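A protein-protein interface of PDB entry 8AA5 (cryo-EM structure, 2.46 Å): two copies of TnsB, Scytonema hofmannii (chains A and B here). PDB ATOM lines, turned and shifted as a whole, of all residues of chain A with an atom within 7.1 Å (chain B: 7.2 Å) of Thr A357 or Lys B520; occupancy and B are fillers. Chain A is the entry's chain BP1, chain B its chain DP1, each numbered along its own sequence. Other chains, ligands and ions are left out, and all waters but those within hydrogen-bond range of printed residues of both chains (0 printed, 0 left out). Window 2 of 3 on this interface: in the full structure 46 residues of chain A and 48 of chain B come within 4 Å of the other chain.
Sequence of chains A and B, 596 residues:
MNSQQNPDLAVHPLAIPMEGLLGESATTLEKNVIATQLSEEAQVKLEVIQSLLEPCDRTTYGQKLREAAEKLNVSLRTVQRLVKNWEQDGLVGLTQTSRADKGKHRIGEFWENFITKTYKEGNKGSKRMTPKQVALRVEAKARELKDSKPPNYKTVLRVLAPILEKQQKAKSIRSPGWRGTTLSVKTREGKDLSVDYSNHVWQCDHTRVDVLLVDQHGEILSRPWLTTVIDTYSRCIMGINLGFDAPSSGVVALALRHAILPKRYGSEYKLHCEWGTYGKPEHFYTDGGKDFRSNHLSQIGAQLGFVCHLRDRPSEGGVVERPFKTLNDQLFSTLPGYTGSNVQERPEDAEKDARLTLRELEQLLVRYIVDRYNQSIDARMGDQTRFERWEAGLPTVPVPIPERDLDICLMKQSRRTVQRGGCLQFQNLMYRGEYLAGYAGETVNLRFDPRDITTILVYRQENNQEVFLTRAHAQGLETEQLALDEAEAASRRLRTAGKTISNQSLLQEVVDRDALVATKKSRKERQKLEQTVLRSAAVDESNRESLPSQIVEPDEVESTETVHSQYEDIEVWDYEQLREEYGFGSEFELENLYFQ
Of the 9 printed residues of chain B, 5 touch a printed residue of chain A. Printed residues of chain B that touch a printed residue of chain A: Leu B516, Val B517, Lys B520, Lys B521 and Ser B522. Hydrophobic or aromatic side chains of chain B within 4 Å of the printed part of chain A: Leu B516 and Val B517. Printed residues of chain A that touch a printed residue of chain B: Pro A336, Arg A355, Leu A356, Thr A357, Glu A360 and Leu A364. Hydrophobic or aromatic side chains of chain A within 4 Å of the printed part of chain B: Pro A336, Leu A356 and Leu A364.
The backbone carbonyl oxygen of Arg A355 lies within hydrogen-bond range of the side-chain amino group of Lys B520 (2.4 Å). OG of Ser B522 lies within hydrogen-bond range of NH2 of Arg A355, 3.0 Å away.
Val B517 touches Pro A336. CB of Arg A355 touches O of Lys B521 (3.2 Å). CD2 of Leu B516 touches CD2 of Leu A356 (3.9 Å). Lys B520 touches Leu A356. Thr A357 touches Lys B520. OE1 of Glu A360 touches CD2 of Leu B516, 3.8 Å away. Lys B520 touches Glu A360 (CE to OE1, 3.2 Å). CD2 of Leu A364 touches CD1 of Leu B516, 3.8 Å away.
Thr A357 touches just one residue of chain B: Lys B520 (3.8 Å). Lys B520 touches just these residues of chain A: Arg A355 (2.4 Å), Leu A356 (3.9 Å), Thr A357 (3.8 Å) and Glu A360 (3.2 Å). Of the printed residues of chain B, Leu A356 touches Leu B516 and Lys B520. Printed residues of chain B within 4 Å of Leu A364: Leu B516. Of the printed residues of chain A, Leu B516 touches Leu A356 (3.9 Å), Glu A360 (3.8 Å) and Leu A364 (3.8 Å). Of the printed residues of chain A, Lys B521 touches Arg A355 (3.2 Å). Of the printed residues of chain A, Val B517 touches Pro A336 (3.9 Å). Leu A212 touches none of the printed residues of chain B. Ala A354 touches none of the printed residues of chain B. The nearest printed residue of chain B that does not touch Thr A357 is Leu B516 (7.5 Å). The nearest residue of chain A that does not touch Lys B520 is Val A214 (4.3 Å). The nearest printed residue of chain A that does not touch Val B517 is Arg A355 (4.7 Å).
OG1 of Thr B519 is in hydrogen-bond range of O of Leu B516, at 3.1 Å. The backbone NH of Val A214 sits at hydrogen-bond distance from the backbone carbonyl oxygen of Leu A356 (2.4 Å). The side-chain hydroxyl (OG1) of Thr A357 lies within hydrogen-bond range of the backbone NH (N) of Glu A360 (3.2 Å). OG1 of Thr A357 sits at hydrogen-bond distance from N of Arg A359 (3.2 Å).
No position is printed for both chains.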
ATOM      1  N   VAL A 211      -3.910  -4.989 -14.811  1.00  0.00           N
ATOM      2  CA  VAL A 211      -4.521  -3.945 -13.999  1.00  0.00           C
ATOM      3  C   VAL A 211      -3.498  -2.839 -13.788  1.00  0.00           C
ATOM      4  O   VAL A 211      -2.387  -3.096 -13.307  1.00  0.00           O
ATOM      5  CB  VAL A 211      -5.026  -4.495 -12.656  1.00  0.00           C
ATOM      6  CG1 VAL A 211      -5.263  -3.368 -11.663  1.00  0.00           C
ATOM      7  CG2 VAL A 211      -6.295  -5.303 -12.867  1.00  0.00           C
ATOM      8  N   LEU A 212      -3.869  -1.612 -14.149  1.00  0.00           N
ATOM      9  CA  LEU A 212      -3.016  -0.456 -13.913  1.00  0.00           C
ATOM     10  C   LEU A 212      -3.131  -0.001 -12.465  1.00  0.00           C
ATOM     11  O   LEU A 212      -4.217  -0.016 -11.879  1.00  0.00           O
ATOM     12  CB  LEU A 212      -3.387   0.694 -14.849  1.00  0.00           C
ATOM     13  CG  LEU A 212      -2.966   0.593 -16.315  1.00  0.00           C
ATOM     14  CD1 LEU A 212      -3.702   1.627 -17.147  1.00  0.00           C
ATOM     15  CD2 LEU A 212      -1.466   0.759 -16.458  1.00  0.00           C
ATOM     16  N   LEU A 213      -2.004   0.405 -11.891  1.00  0.00           N
ATOM     17  CA  LEU A 213      -1.934   0.804 -10.496  1.00  0.00           C
ATOM     18  C   LEU A 213      -1.518   2.263 -10.381  1.00  0.00           C
ATOM     19  O   LEU A 213      -0.931   2.839 -11.300  1.00  0.00           O
ATOM     20  CB  LEU A 213      -0.951  -0.069  -9.716  1.00  0.00           C
ATOM     21  CG  LEU A 213      -1.014  -1.564  -9.998  1.00  0.00           C
ATOM     22  CD1 LEU A 213       0.013  -2.284  -9.154  1.00  0.00           C
ATOM     23  CD2 LEU A 213      -2.407  -2.081  -9.717  1.00  0.00           C
ATOM     24  N   VAL A 214      -1.832   2.855  -9.228  1.00  0.00           N
ATOM     25  CA  VAL A 214      -1.466   4.232  -8.932  1.00  0.00           C
ATOM     26  C   VAL A 214      -0.728   4.277  -7.603  1.00  0.00           C
ATOM     27  O   VAL A 214      -0.872   3.399  -6.750  1.00  0.00           O
ATOM     28  CB  VAL A 214      -2.686   5.174  -8.898  1.00  0.00           C
ATOM     29  CG1 VAL A 214      -3.618   4.876 -10.050  1.00  0.00           C
ATOM     30  CG2 VAL A 214      -3.413   5.063  -7.570  1.00  0.00           C
ATOM     31  N   ASP A 215       0.090   5.314  -7.447  1.00  0.00           N
ATOM     32  CA  ASP A 215       0.837   5.535  -6.219  1.00  0.00           C
ATOM     33  C   ASP A 215       0.027   6.439  -5.293  1.00  0.00           C
ATOM     34  O   ASP A 215      -1.171   6.657  -5.490  1.00  0.00           O
ATOM     35  CB  ASP A 215       2.217   6.112  -6.527  1.00  0.00           C
ATOM     36  CG  ASP A 215       2.171   7.242  -7.533  1.00  0.00           C
ATOM     37  OD1 ASP A 215       1.110   7.887  -7.661  1.00  0.00           O
ATOM     38  OD2 ASP A 215       3.199   7.487  -8.197  1.00  0.00           O
ATOM     39  N   GLN A 216       0.678   6.965  -4.259  1.00  0.00           N
ATOM     40  CA  GLN A 216       0.009   7.865  -3.333  1.00  0.00           C
ATOM     41  C   GLN A 216      -0.457   9.127  -4.050  1.00  0.00           C
ATOM     42  O   GLN A 216       0.181   9.605  -4.992  1.00  0.00           O
ATOM     43  CB  GLN A 216       0.944   8.230  -2.182  1.00  0.00           C
ATOM     44  CG  GLN A 216       1.765   7.068  -1.657  1.00  0.00           C
ATOM     45  CD  GLN A 216       3.155   7.017  -2.260  1.00  0.00           C
ATOM     46  OE1 GLN A 216       3.317   7.053  -3.480  1.00  0.00           O
ATOM     47  NE2 GLN A 216       4.169   6.934  -1.406  1.00  0.00           N
ATOM     48  N   GLY A 218      -2.512   9.605  -6.143  1.00  0.00           N
ATOM     49  CA  GLY A 218      -3.103   9.303  -7.431  1.00  0.00           C
ATOM     50  C   GLY A 218      -2.218   9.650  -8.611  1.00  0.00           C
ATOM     51  O   GLY A 218      -2.166  10.808  -9.037  1.00  0.00           O
ATOM     52  N   LEU A 221       1.611   4.257 -12.387  1.00  0.00           N
ATOM     53  CA  LEU A 221       3.013   3.877 -12.487  1.00  0.00           C
ATOM     54  C   LEU A 221       3.259   2.866 -13.599  1.00  0.00           C
ATOM     55  O   LEU A 221       3.988   3.160 -14.551  1.00  0.00           O
ATOM     56  CB  LEU A 221       3.507   3.310 -11.151  1.00  0.00           C
ATOM     57  CG  LEU A 221       2.953   3.909  -9.864  1.00  0.00           C
ATOM     58  CD1 LEU A 221       1.995   2.934  -9.213  1.00  0.00           C
ATOM     59  CD2 LEU A 221       4.091   4.246  -8.924  1.00  0.00           C
ATOM     60  N   LEU A 242       3.891 -10.171  -6.268  1.00  0.00           N
ATOM     61  CA  LEU A 242       3.306  -9.115  -7.081  1.00  0.00           C
ATOM     62  C   LEU A 242       4.104  -7.838  -6.865  1.00  0.00           C
ATOM     63  O   LEU A 242       4.198  -7.348  -5.734  1.00  0.00           O
ATOM     64  CB  LEU A 242       1.837  -8.909  -6.720  1.00  0.00           C
ATOM     65  CG  LEU A 242       1.079  -7.824  -7.475  1.00  0.00           C
ATOM     66  CD1 LEU A 242       0.663  -8.333  -8.836  1.00  0.00           C
ATOM     67  CD2 LEU A 242      -0.129  -7.383  -6.675  1.00  0.00           C
ATOM     68  N   PHE A 244       6.340  -4.332  -9.168  1.00  0.00           N
ATOM     69  CA  PHE A 244       6.751  -3.675 -10.403  1.00  0.00           C
ATOM     70  C   PHE A 244       8.098  -4.164 -10.912  1.00  0.00           C
ATOM     71  O   PHE A 244       8.395  -3.985 -12.097  1.00  0.00           O
ATOM     72  CB  PHE A 244       6.803  -2.161 -10.204  1.00  0.00           C
ATOM     73  CG  PHE A 244       5.509  -1.570  -9.737  1.00  0.00           C
ATOM     74  CD1 PHE A 244       4.433  -1.467 -10.596  1.00  0.00           C
ATOM     75  CD2 PHE A 244       5.369  -1.119  -8.439  1.00  0.00           C
ATOM     76  CE1 PHE A 244       3.242  -0.924 -10.170  1.00  0.00           C
ATOM     77  CE2 PHE A 244       4.178  -0.574  -8.009  1.00  0.00           C
ATOM     78  CZ  PHE A 244       3.115  -0.478  -8.875  1.00  0.00           C
ATOM     79  N   PRO A 336     -11.070  -1.484 -11.350  1.00  0.00           N
ATOM     80  CA  PRO A 336     -11.245  -0.206 -12.054  1.00  0.00           C
ATOM     81  C   PRO A 336     -10.255   0.025 -13.183  1.00  0.00           C
ATOM     82  O   PRO A 336     -10.662   0.193 -14.336  1.00  0.00           O
ATOM     83  CB  PRO A 336     -11.058   0.825 -10.937  1.00  0.00           C
ATOM     84  CG  PRO A 336     -11.490   0.118  -9.712  1.00  0.00           C
ATOM     85  CD  PRO A 336     -11.086  -1.313  -9.889  1.00  0.00           C
ATOM     86  N   ALA A 354      -7.669   4.046 -13.955  1.00  0.00           N
ATOM     87  CA  ALA A 354      -6.629   3.480 -13.101  1.00  0.00           C
ATOM     88  C   ALA A 354      -6.632   4.189 -11.754  1.00  0.00           C
ATOM     89  O   ALA A 354      -6.309   5.379 -11.670  1.00  0.00           O
ATOM     90  CB  ALA A 354      -5.269   3.599 -13.779  1.00  0.00           C
ATOM     91  N   ARG A 355      -7.008   3.468 -10.700  1.00  0.00           N
ATOM     92  CA  ARG A 355      -7.078   4.066  -9.371  1.00  0.00           C
ATOM     93  C   ARG A 355      -6.513   3.211  -8.248  1.00  0.00           C
ATOM     94  O   ARG A 355      -6.270   3.755  -7.166  1.00  0.00           O
ATOM     95  CB  ARG A 355      -8.526   4.427  -9.027  1.00  0.00           C
ATOM     96  CG  ARG A 355      -9.356   3.266  -8.523  1.00  0.00           C
ATOM     97  CD  ARG A 355     -10.837   3.551  -8.677  1.00  0.00           C
ATOM     98  NE  ARG A 355     -11.154   4.071  -9.999  1.00  0.00           N
ATOM     99  CZ  ARG A 355     -12.372   4.408 -10.400  1.00  0.00           C
ATOM    100  NH1 ARG A 355     -13.420   4.284  -9.603  1.00  0.00           N
ATOM    101  NH2 ARG A 355     -12.542   4.885 -11.630  1.00  0.00           N
ATOM    102  N   LEU A 356      -6.284   1.915  -8.438  1.00  0.00           N
ATOM    103  CA  LEU A 356      -5.833   1.083  -7.332  1.00  0.00           C
ATOM    104  C   LEU A 356      -4.326   1.211  -7.132  1.00  0.00           C
ATOM    105  O   LEU A 356      -3.590   1.672  -8.008  1.00  0.00           O
ATOM    106  CB  LEU A 356      -6.203  -0.382  -7.564  1.00  0.00           C
ATOM    107  CG  LEU A 356      -7.584  -0.825  -7.080  1.00  0.00           C
ATOM    108  CD1 LEU A 356      -8.158  -1.880  -7.995  1.00  0.00           C
ATOM    109  CD2 LEU A 356      -7.519  -1.334  -5.655  1.00  0.00           C
ATOM    110  N   THR A 357      -3.873   0.803  -5.952  1.00  0.00           N
ATOM    111  CA  THR A 357      -2.461   0.792  -5.601  1.00  0.00           C
ATOM    112  C   THR A 357      -1.940  -0.640  -5.589  1.00  0.00           C
ATOM    113  O   THR A 357      -2.702  -1.606  -5.673  1.00  0.00           O
ATOM    114  CB  THR A 357      -2.231   1.453  -4.236  1.00  0.00           C
ATOM    115  OG1 THR A 357      -2.295   0.462  -3.205  1.00  0.00           O
ATOM    116  CG2 THR A 357      -3.288   2.510  -3.973  1.00  0.00           C
ATOM    117  N   LEU A 358      -0.615  -0.767  -5.487  1.00  0.00           N
ATOM    118  CA  LEU A 358      -0.010  -2.093  -5.424  1.00  0.00           C
ATOM    119  C   LEU A 358      -0.420  -2.830  -4.155  1.00  0.00           C
ATOM    120  O   LEU A 358      -0.672  -4.040  -4.187  1.00  0.00           O
ATOM    121  CB  LEU A 358       1.511  -1.987  -5.511  1.00  0.00           C
ATOM    122  CG  LEU A 358       2.256  -3.321  -5.503  1.00  0.00           C
ATOM    123  CD1 LEU A 358       1.752  -4.226  -6.610  1.00  0.00           C
ATOM    124  CD2 LEU A 358       3.750  -3.111  -5.627  1.00  0.00           C
ATOM    125  N   ARG A 359      -0.488  -2.120  -3.029  1.00  0.00           N
ATOM    126  CA  ARG A 359      -0.856  -2.757  -1.769  1.00  0.00           C
ATOM    127  C   ARG A 359      -2.294  -3.264  -1.797  1.00  0.00           C
ATOM    128  O   ARG A 359      -2.574  -4.385  -1.356  1.00  0.00           O
ATOM    129  CB  ARG A 359      -0.651  -1.775  -0.615  1.00  0.00           C
ATOM    130  CG  ARG A 359      -1.461  -2.081   0.629  1.00  0.00           C
ATOM    131  CD  ARG A 359      -1.219  -1.037   1.703  1.00  0.00           C
ATOM    132  NE  ARG A 359      -0.163  -1.437   2.626  1.00  0.00           N
ATOM    133  CZ  ARG A 359       0.101  -0.824   3.772  1.00  0.00           C
ATOM    134  NH1 ARG A 359      -0.598   0.226   4.171  1.00  0.00           N
ATOM    135  NH2 ARG A 359       1.091  -1.276   4.535  1.00  0.00           N
ATOM    136  N   GLU A 360      -3.219  -2.456  -2.315  1.00  0.00           N
ATOM    137  CA  GLU A 360      -4.611  -2.884  -2.379  1.00  0.00           C
ATOM    138  C   GLU A 360      -4.793  -4.015  -3.383  1.00  0.00           C
ATOM    139  O   GLU A 360      -5.583  -4.939  -3.149  1.00  0.00           O
ATOM    140  CB  GLU A 360      -5.505  -1.698  -2.728  1.00  0.00           C
ATOM    141  CG  GLU A 360      -5.249  -0.467  -1.879  1.00  0.00           C
ATOM    142  CD  GLU A 360      -6.505   0.343  -1.634  1.00  0.00           C
ATOM    143  OE1 GLU A 360      -7.317   0.478  -2.571  1.00  0.00           O
ATOM    144  OE2 GLU A 360      -6.678   0.846  -0.503  1.00  0.00           O
ATOM    145  N   LEU A 361      -4.070  -3.961  -4.503  1.00  0.00           N
ATOM    146  CA  LEU A 361      -4.106  -5.070  -5.450  1.00  0.00           C
ATOM    147  C   LEU A 361      -3.583  -6.348  -4.813  1.00  0.00           C
ATOM    148  O   LEU A 361      -4.130  -7.430  -5.044  1.00  0.00           O
ATOM    149  CB  LEU A 361      -3.298  -4.731  -6.701  1.00  0.00           C
ATOM    150  CG  LEU A 361      -3.331  -5.835  -7.762  1.00  0.00           C
ATOM    151  CD1 LEU A 361      -4.736  -6.011  -8.295  1.00  0.00           C
ATOM    152  CD2 LEU A 361      -2.362  -5.553  -8.889  1.00  0.00           C
ATOM    153  N   GLU A 362      -2.522  -6.244  -4.010  1.00  0.00           N
ATOM    154  CA  GLU A 362      -2.002  -7.417  -3.318  1.00  0.00           C
ATOM    155  C   GLU A 362      -3.012  -7.955  -2.316  1.00  0.00           C
ATOM    156  O   GLU A 362      -3.167  -9.173  -2.179  1.00  0.00           O
ATOM    157  CB  GLU A 362      -0.684  -7.080  -2.624  1.00  0.00           C
ATOM    158  CG  GLU A 362       0.202  -8.285  -2.371  1.00  0.00           C
ATOM    159  CD  GLU A 362       0.303  -8.637  -0.901  1.00  0.00           C
ATOM    160  OE1 GLU A 362       0.251  -7.713  -0.063  1.00  0.00           O
ATOM    161  OE2 GLU A 362       0.433  -9.838  -0.584  1.00  0.00           O
ATOM    162  N   GLN A 363      -3.708  -7.065  -1.606  1.00  0.00           N
ATOM    163  CA  GLN A 363      -4.753  -7.502  -0.684  1.00  0.00           C
ATOM    164  C   GLN A 363      -5.842  -8.275  -1.418  1.00  0.00           C
ATOM    165  O   GLN A 363      -6.224  -9.382  -1.011  1.00  0.00           O
ATOM    166  CB  GLN A 363      -5.358  -6.296   0.034  1.00  0.00           C
ATOM    167  CG  GLN A 363      -4.455  -5.655   1.066  1.00  0.00           C
ATOM    168  CD  GLN A 363      -5.234  -4.876   2.099  1.00  0.00           C
ATOM    169  OE1 GLN A 363      -6.448  -5.025   2.221  1.00  0.00           O
ATOM    170  NE2 GLN A 363      -4.537  -4.039   2.857  1.00  0.00           N
ATOM    171  N   LEU A 364      -6.345  -7.705  -2.515  1.00  0.00           N
ATOM    172  CA  LEU A 364      -7.390  -8.368  -3.286  1.00  0.00           C
ATOM    173  C   LEU A 364      -6.906  -9.700  -3.847  1.00  0.00           C
ATOM    174  O   LEU A 364      -7.629 -10.701  -3.797  1.00  0.00           O
ATOM    175  CB  LEU A 364      -7.871  -7.456  -4.413  1.00  0.00           C
ATOM    176  CG  LEU A 364      -8.447  -6.101  -4.014  1.00  0.00           C
ATOM    177  CD1 LEU A 364      -8.451  -5.160  -5.201  1.00  0.00           C
ATOM    178  CD2 LEU A 364      -9.847  -6.261  -3.456  1.00  0.00           C
ATOM    179  N   ASP B 514     -16.106  -5.815  -4.241  1.00  0.00           N
ATOM    180  CA  ASP B 514     -17.006  -4.776  -4.733  1.00  0.00           C
ATOM    181  C   ASP B 514     -16.994  -3.562  -3.812  1.00  0.00           C
ATOM    182  O   ASP B 514     -16.940  -2.418  -4.276  1.00  0.00           O
ATOM    183  CB  ASP B 514     -18.424  -5.326  -4.865  1.00  0.00           C
ATOM    184  CG  ASP B 514     -18.698  -5.918  -6.230  1.00  0.00           C
ATOM    185  OD1 ASP B 514     -17.768  -5.949  -7.064  1.00  0.00           O
ATOM    186  OD2 ASP B 514     -19.843  -6.352  -6.469  1.00  0.00           O
ATOM    187  N   ALA B 515     -17.039  -3.797  -2.500  1.00  0.00           N
ATOM    188  CA  ALA B 515     -17.000  -2.690  -1.553  1.00  0.00           C
ATOM    189  C   ALA B 515     -15.691  -1.917  -1.655  1.00  0.00           C
ATOM    190  O   ALA B 515     -15.691  -0.681  -1.643  1.00  0.00           O
ATOM    191  CB  ALA B 515     -17.206  -3.208  -0.130  1.00  0.00           C
ATOM    192  N   LEU B 516     -14.565  -2.627  -1.762  1.00  0.00           N
ATOM    193  CA  LEU B 516     -13.266  -1.964  -1.808  1.00  0.00           C
ATOM    194  C   LEU B 516     -13.120  -1.120  -3.065  1.00  0.00           C
ATOM    195  O   LEU B 516     -12.603   0.001  -3.006  1.00  0.00           O
ATOM    196  CB  LEU B 516     -12.144  -2.999  -1.713  1.00  0.00           C
ATOM    197  CG  LEU B 516     -10.699  -2.519  -1.520  1.00  0.00           C
ATOM    198  CD1 LEU B 516      -9.898  -3.581  -0.786  1.00  0.00           C
ATOM    199  CD2 LEU B 516     -10.021  -2.182  -2.841  1.00  0.00           C
ATOM    200  N   VAL B 517     -13.559  -1.637  -4.215  1.00  0.00           N
ATOM    201  CA  VAL B 517     -13.496  -0.831  -5.427  1.00  0.00           C
ATOM    202  C   VAL B 517     -14.531   0.285  -5.407  1.00  0.00           C
ATOM    203  O   VAL B 517     -14.380   1.276  -6.130  1.00  0.00           O
ATOM    204  CB  VAL B 517     -13.656  -1.703  -6.688  1.00  0.00           C
ATOM    205  CG1 VAL B 517     -12.644  -2.840  -6.679  1.00  0.00           C
ATOM    206  CG2 VAL B 517     -15.070  -2.239  -6.803  1.00  0.00           C
ATOM    207  N   ALA B 518     -15.582   0.156  -4.591  1.00  0.00           N
ATOM    208  CA  ALA B 518     -16.586   1.213  -4.507  1.00  0.00           C
ATOM    209  C   ALA B 518     -16.063   2.424  -3.743  1.00  0.00           C
ATOM    210  O   ALA B 518     -16.364   3.567  -4.102  1.00  0.00           O
ATOM    211  CB  ALA B 518     -17.860   0.678  -3.857  1.00  0.00           C
ATOM    212  N   THR B 519     -15.280   2.198  -2.686  1.00  0.00           N
ATOM    213  CA  THR B 519     -14.792   3.313  -1.883  1.00  0.00           C
ATOM    214  C   THR B 519     -13.714   4.113  -2.602  1.00  0.00           C
ATOM    215  O   THR B 519     -13.606   5.327  -2.393  1.00  0.00           O
ATOM    216  CB  THR B 519     -14.247   2.817  -0.543  1.00  0.00           C
ATOM    217  OG1 THR B 519     -12.999   2.144  -0.751  1.00  0.00           O
ATOM    218  CG2 THR B 519     -15.234   1.877   0.128  1.00  0.00           C
ATOM    219  N   LYS B 520     -12.911   3.463  -3.439  1.00  0.00           N
ATOM    220  CA  LYS B 520     -11.738   4.121  -3.994  1.00  0.00           C
ATOM    221  C   LYS B 520     -12.143   5.175  -5.019  1.00  0.00           C
ATOM    222  O   LYS B 520     -13.143   5.037  -5.728  1.00  0.00           O
ATOM    223  CB  LYS B 520     -10.798   3.094  -4.620  1.00  0.00           C
ATOM    224  CG  LYS B 520      -9.739   2.599  -3.646  1.00  0.00           C
ATOM    225  CD  LYS B 520      -8.571   3.558  -3.535  1.00  0.00           C
ATOM    226  CE  LYS B 520      -7.415   3.119  -4.405  1.00  0.00           C
ATOM    227  NZ  LYS B 520      -6.570   4.269  -4.829  1.00  0.00           N
ATOM    228  N   LYS B 521     -11.350   6.240  -5.085  1.00  0.00           N
ATOM    229  CA  LYS B 521     -11.662   7.425  -5.871  1.00  0.00           C
ATOM    230  C   LYS B 521     -10.908   7.412  -7.196  1.00  0.00           C
ATOM    231  O   LYS B 521      -9.850   6.791  -7.325  1.00  0.00           O
ATOM    232  CB  LYS B 521     -11.314   8.692  -5.086  1.00  0.00           C
ATOM    233  CG  LYS B 521     -11.982   9.962  -5.586  1.00  0.00           C
ATOM    234  CD  LYS B 521     -10.949  11.001  -5.993  1.00  0.00           C
ATOM    235  CE  LYS B 521     -10.234  11.584  -4.787  1.00  0.00           C
ATOM    236  NZ  LYS B 521      -9.226  12.604  -5.189  1.00  0.00           N
ATOM    237  N   SER B 522     -11.464   8.116  -8.179  1.00  0.00           N
ATOM    238  CA  SER B 522     -10.848   8.246  -9.494  1.00  0.00           C
ATOM    239  C   SER B 522      -9.737   9.293  -9.431  1.00  0.00           C
ATOM    240  O   SER B 522      -9.295   9.703  -8.353  1.00  0.00           O
ATOM    241  CB  SER B 522     -11.904   8.596 -10.538  1.00  0.00           C
ATOM    242  OG  SER B 522     -12.957   7.649 -10.537  1.00  0.00           O
